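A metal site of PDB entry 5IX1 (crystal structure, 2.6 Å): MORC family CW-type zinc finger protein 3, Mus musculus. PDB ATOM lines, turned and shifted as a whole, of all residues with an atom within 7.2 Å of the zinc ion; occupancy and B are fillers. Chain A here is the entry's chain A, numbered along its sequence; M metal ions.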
ATOM      1  N   GLN A 407      18.951  -2.372  10.422  1.00  0.00           N
ATOM      2  CA  GLN A 407      18.765  -2.805  11.783  1.00  0.00           C
ATOM      3  C   GLN A 407      17.367  -2.449  12.159  1.00  0.00           C
ATOM      4  O   GLN A 407      16.892  -1.385  11.850  1.00  0.00           O
ATOM      5  CB  GLN A 407      19.766  -2.117  12.686  1.00  0.00           C
ATOM      6  CG  GLN A 407      19.153  -1.140  13.669  1.00  0.00           C
ATOM      7  CD  GLN A 407      20.196  -0.321  14.362  1.00  0.00           C
ATOM      8  OE1 GLN A 407      20.868   0.519  13.752  1.00  0.00           O
ATOM      9  NE2 GLN A 407      20.355  -0.545  15.643  1.00  0.00           N
ATOM     10  N   CYS A 408      16.693  -3.381  12.790  1.00  0.00           N
ATOM     11  CA  CYS A 408      15.379  -3.130  13.330  1.00  0.00           C
ATOM     12  C   CYS A 408      15.467  -2.249  14.556  1.00  0.00           C
ATOM     13  O   CYS A 408      16.334  -2.441  15.396  1.00  0.00           O
ATOM     14  CB  CYS A 408      14.674  -4.438  13.688  1.00  0.00           C
ATOM     15  SG  CYS A 408      13.047  -4.120  14.381  1.00  0.00           S
ATOM     16  N   ASP A 409      14.612  -1.254  14.575  1.00  0.00           N
ATOM     17  CA  ASP A 409      14.490  -0.318  15.642  1.00  0.00           C
ATOM     18  C   ASP A 409      13.896  -0.920  16.913  1.00  0.00           C
ATOM     19  O   ASP A 409      14.043  -0.361  17.963  1.00  0.00           O
ATOM     20  CB  ASP A 409      13.739   0.922  15.190  1.00  0.00           C
ATOM     21  CG  ASP A 409      14.550   1.745  14.227  1.00  0.00           C
ATOM     22  OD1 ASP A 409      15.750   1.538  14.136  1.00  0.00           O
ATOM     23  OD2 ASP A 409      14.000   2.614  13.545  1.00  0.00           O
ATOM     24  N   ALA A 410      13.172  -2.006  16.791  1.00  0.00           N
ATOM     25  CA  ALA A 410      12.618  -2.671  17.958  1.00  0.00           C
ATOM     26  C   ALA A 410      13.071  -4.090  18.263  1.00  0.00           C
ATOM     27  O   ALA A 410      12.426  -4.758  19.024  1.00  0.00           O
ATOM     28  CB  ALA A 410      11.123  -2.615  17.912  1.00  0.00           C
ATOM     29  N   CYS A 411      14.123  -4.575  17.632  1.00  0.00           N
ATOM     30  CA  CYS A 411      14.855  -5.764  18.107  1.00  0.00           C
ATOM     31  C   CYS A 411      16.306  -5.425  18.298  1.00  0.00           C
ATOM     32  O   CYS A 411      16.998  -6.087  19.075  1.00  0.00           O
ATOM     33  CB  CYS A 411      14.852  -6.919  17.114  1.00  0.00           C
ATOM     34  SG  CYS A 411      13.474  -7.089  15.998  1.00  0.00           S
ATOM     35  N   LEU A 412      16.728  -4.513  17.444  1.00  0.00           N
ATOM     36  CA  LEU A 412      18.113  -4.215  17.209  1.00  0.00           C
ATOM     37  C   LEU A 412      18.737  -5.260  16.313  1.00  0.00           C
ATOM     38  O   LEU A 412      19.918  -5.242  16.063  1.00  0.00           O
ATOM     39  CB  LEU A 412      18.857  -4.151  18.526  1.00  0.00           C
ATOM     40  CG  LEU A 412      19.197  -2.739  18.938  1.00  0.00           C
ATOM     41  CD1 LEU A 412      17.986  -1.836  18.789  1.00  0.00           C
ATOM     42  CD2 LEU A 412      19.655  -2.764  20.381  1.00  0.00           C
ATOM     43  N   LYS A 413      17.909  -6.184  15.836  1.00  0.00           N
ATOM     44  CA  LYS A 413      18.329  -7.244  14.949  1.00  0.00           C
ATOM     45  C   LYS A 413      18.626  -6.697  13.571  1.00  0.00           C
ATOM     46  O   LYS A 413      18.012  -5.738  13.141  1.00  0.00           O
ATOM     47  CB  LYS A 413      17.252  -8.297  14.845  1.00  0.00           C
ATOM     48  CG  LYS A 413      16.889  -9.000  16.135  1.00  0.00           C
ATOM     49  CD  LYS A 413      16.969 -10.499  15.954  1.00  0.00           C
ATOM     50  CE  LYS A 413      17.249 -11.211  17.254  1.00  0.00           C
ATOM     51  NZ  LYS A 413      16.079 -11.195  18.174  1.00  0.00           N
ATOM     52  N   ARG A 415      18.447  -7.195   9.615  1.00  0.00           N
ATOM     53  CA  ARG A 415      17.736  -7.966   8.630  1.00  0.00           C
ATOM     54  C   ARG A 415      18.227  -7.598   7.243  1.00  0.00           C
ATOM     55  O   ARG A 415      18.458  -6.440   6.959  1.00  0.00           O
ATOM     56  CB  ARG A 415      16.233  -7.759   8.751  1.00  0.00           C
ATOM     57  CG  ARG A 415      15.631  -8.076  10.100  1.00  0.00           C
ATOM     58  CD  ARG A 415      15.796  -9.507  10.545  1.00  0.00           C
ATOM     59  NE  ARG A 415      14.687  -9.911  11.385  1.00  0.00           N
ATOM     60  CZ  ARG A 415      14.680 -11.003  12.133  1.00  0.00           C
ATOM     61  NH1 ARG A 415      15.725 -11.792  12.159  1.00  0.00           N
ATOM     62  NH2 ARG A 415      13.637 -11.299  12.873  1.00  0.00           N
ATOM     63  N   TRP A 428      12.761   1.704  10.677  1.00  0.00           N
ATOM     64  CA  TRP A 428      12.385   0.449  10.061  1.00  0.00           C
ATOM     65  C   TRP A 428      12.257  -0.675  11.077  1.00  0.00           C
ATOM     66  O   TRP A 428      13.136  -0.898  11.863  1.00  0.00           O
ATOM     67  CB  TRP A 428      13.460   0.103   9.041  1.00  0.00           C
ATOM     68  CG  TRP A 428      13.194  -1.028   8.132  1.00  0.00           C
ATOM     69  CD1 TRP A 428      12.781  -0.955   6.852  1.00  0.00           C
ATOM     70  CD2 TRP A 428      13.368  -2.412   8.414  1.00  0.00           C
ATOM     71  NE1 TRP A 428      12.666  -2.206   6.325  1.00  0.00           N
ATOM     72  CE2 TRP A 428      13.022  -3.121   7.273  1.00  0.00           C
ATOM     73  CE3 TRP A 428      13.761  -3.120   9.538  1.00  0.00           C
ATOM     74  CZ2 TRP A 428      13.068  -4.485   7.206  1.00  0.00           C
ATOM     75  CZ3 TRP A 428      13.809  -4.475   9.467  1.00  0.00           C
ATOM     76  CH2 TRP A 428      13.463  -5.143   8.318  1.00  0.00           C
ATOM     77  N   TYR A 429      11.152  -1.402  11.018  1.00  0.00           N
ATOM     78  CA  TYR A 429      10.841  -2.418  12.021  1.00  0.00           C
ATOM     79  C   TYR A 429      10.625  -3.769  11.351  1.00  0.00           C
ATOM     80  O   TYR A 429      10.224  -3.817  10.208  1.00  0.00           O
ATOM     81  CB  TYR A 429       9.591  -2.009  12.822  1.00  0.00           C
ATOM     82  CG  TYR A 429       9.666  -0.603  13.371  1.00  0.00           C
ATOM     83  CD1 TYR A 429       9.195   0.482  12.641  1.00  0.00           C
ATOM     84  CD2 TYR A 429      10.212  -0.354  14.622  1.00  0.00           C
ATOM     85  CE1 TYR A 429       9.269   1.773  13.146  1.00  0.00           C
ATOM     86  CE2 TYR A 429      10.294   0.916  15.133  1.00  0.00           C
ATOM     87  CZ  TYR A 429       9.821   1.982  14.389  1.00  0.00           C
ATOM     88  OH  TYR A 429       9.893   3.255  14.903  1.00  0.00           O
ATOM     89  N   CYS A 430      10.895  -4.863  12.059  1.00  0.00           N
ATOM     90  CA  CYS A 430      10.733  -6.180  11.441  1.00  0.00           C
ATOM     91  C   CYS A 430       9.333  -6.403  10.870  1.00  0.00           C
ATOM     92  O   CYS A 430       9.159  -7.140   9.907  1.00  0.00           O
ATOM     93  CB  CYS A 430      11.066  -7.291  12.445  1.00  0.00           C
ATOM     94  SG  CYS A 430      12.825  -7.694  12.549  1.00  0.00           S
ATOM     95  N   SER A 431       8.356  -5.708  11.422  1.00  0.00           N
ATOM     96  CA  SER A 431       6.975  -5.851  11.062  1.00  0.00           C
ATOM     97  C   SER A 431       6.693  -5.443   9.649  1.00  0.00           C
ATOM     98  O   SER A 431       5.790  -5.950   9.014  1.00  0.00           O
ATOM     99  CB  SER A 431       6.112  -5.052  11.996  1.00  0.00           C
ATOM    100  OG  SER A 431       5.617  -5.892  13.004  1.00  0.00           O
ATOM    101  N   PHE A 438      11.309 -12.898   7.531  1.00  0.00           N
ATOM    102  CA  PHE A 438      11.753 -12.149   8.686  1.00  0.00           C
ATOM    103  C   PHE A 438      10.856 -10.962   8.896  1.00  0.00           C
ATOM    104  O   PHE A 438      11.253  -9.834   8.745  1.00  0.00           O
ATOM    105  CB  PHE A 438      13.192 -11.692   8.480  1.00  0.00           C
ATOM    106  CG  PHE A 438      14.104 -12.800   8.125  1.00  0.00           C
ATOM    107  CD1 PHE A 438      14.753 -13.510   9.097  1.00  0.00           C
ATOM    108  CD2 PHE A 438      14.313 -13.137   6.810  1.00  0.00           C
ATOM    109  CE1 PHE A 438      15.604 -14.535   8.773  1.00  0.00           C
ATOM    110  CE2 PHE A 438      15.161 -14.157   6.472  1.00  0.00           C
ATOM    111  CZ  PHE A 438      15.806 -14.861   7.456  1.00  0.00           C
ATOM    112  N   ARG A 439       9.613 -11.243   9.219  1.00  0.00           N
ATOM    113  CA  ARG A 439       8.654 -10.202   9.484  1.00  0.00           C
ATOM    114  C   ARG A 439       8.313 -10.145  10.968  1.00  0.00           C
ATOM    115  O   ARG A 439       7.438  -9.430  11.392  1.00  0.00           O
ATOM    116  CB  ARG A 439       7.399 -10.428   8.649  1.00  0.00           C
ATOM    117  CG  ARG A 439       7.525  -9.957   7.216  1.00  0.00           C
ATOM    118  CD  ARG A 439       6.190  -9.933   6.504  1.00  0.00           C
ATOM    119  NE  ARG A 439       6.363  -9.597   5.109  1.00  0.00           N
ATOM    120  CZ  ARG A 439       5.753 -10.217   4.108  1.00  0.00           C
ATOM    121  NH1 ARG A 439       4.926 -11.194   4.349  1.00  0.00           N
ATOM    122  NH2 ARG A 439       5.985  -9.832   2.880  1.00  0.00           N
ATOM    123  N   ASN A 440       9.022 -10.949  11.742  1.00  0.00           N
ATOM    124  CA  ASN A 440       8.805 -11.073  13.158  1.00  0.00           C
ATOM    125  C   ASN A 440      10.040 -10.721  13.944  1.00  0.00           C
ATOM    126  O   ASN A 440      11.097 -11.259  13.719  1.00  0.00           O
ATOM    127  CB  ASN A 440       8.443 -12.502  13.459  1.00  0.00           C
ATOM    128  CG  ASN A 440       7.375 -12.609  14.493  1.00  0.00           C
ATOM    129  OD1 ASN A 440       7.626 -12.385  15.671  1.00  0.00           O
ATOM    130  ND2 ASN A 440       6.172 -12.950  14.068  1.00  0.00           N
ATOM    131  N   CYS A 441       9.887  -9.834  14.916  1.00  0.00           N
ATOM    132  CA  CYS A 441      10.988  -9.426  15.773  1.00  0.00           C
ATOM    133  C   CYS A 441      11.620 -10.651  16.432  1.00  0.00           C
ATOM    134  O   CYS A 441      12.810 -10.659  16.722  1.00  0.00           O
ATOM    135  CB  CYS A 441      10.487  -8.418  16.817  1.00  0.00           C
ATOM    136  SG  CYS A 441      10.094  -6.802  16.112  1.00  0.00           S
ATOM    137  N   GLU A 442      10.814 -11.660  16.640  1.00  0.00           N
ATOM    138  CA  GLU A 442      11.275 -12.855  17.292  1.00  0.00           C
ATOM    139  C   GLU A 442      11.973 -13.782  16.337  1.00  0.00           C
ATOM    140  O   GLU A 442      12.154 -14.946  16.645  1.00  0.00           O
ATOM    141  CB  GLU A 442      10.093 -13.572  17.901  1.00  0.00           C
ATOM    142  CG  GLU A 442       9.707 -13.071  19.284  1.00  0.00           C
ATOM    143  CD  GLU A 442      10.872 -13.010  20.235  1.00  0.00           C
ATOM    144  OE1 GLU A 442      11.421 -14.081  20.569  1.00  0.00           O
ATOM    145  OE2 GLU A 442      11.251 -11.889  20.630  1.00  0.00           O
HETATM  146 ZN    ZN M   1      12.224  -6.067  14.737  1.00  0.00          ZN
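The side-chain sulfur of Cys 430 lies close to the guanidinium group of Arg 415, at 3.1 Å.
The backbone NH of Ala 410 sits close to the side-chain sulfur of Cys 408.
The backbone NH of Cys 408 is in hydrogen-bond range of the backbone carbonyl oxygen of Lys 413 (2.7 Å).
The nearest printed residue that does not touch the zinc ion is Ala 410 (4.1 Å).
The zinc ion is bound by SG of Cys 411 (2.0 Å), SG of Cys 408 (2.1 Å), SG of Cys 441 (2.6 Å) and SG of Cys 430 (2.8 Å).
The zinc ion has four donor atoms within binding distance.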
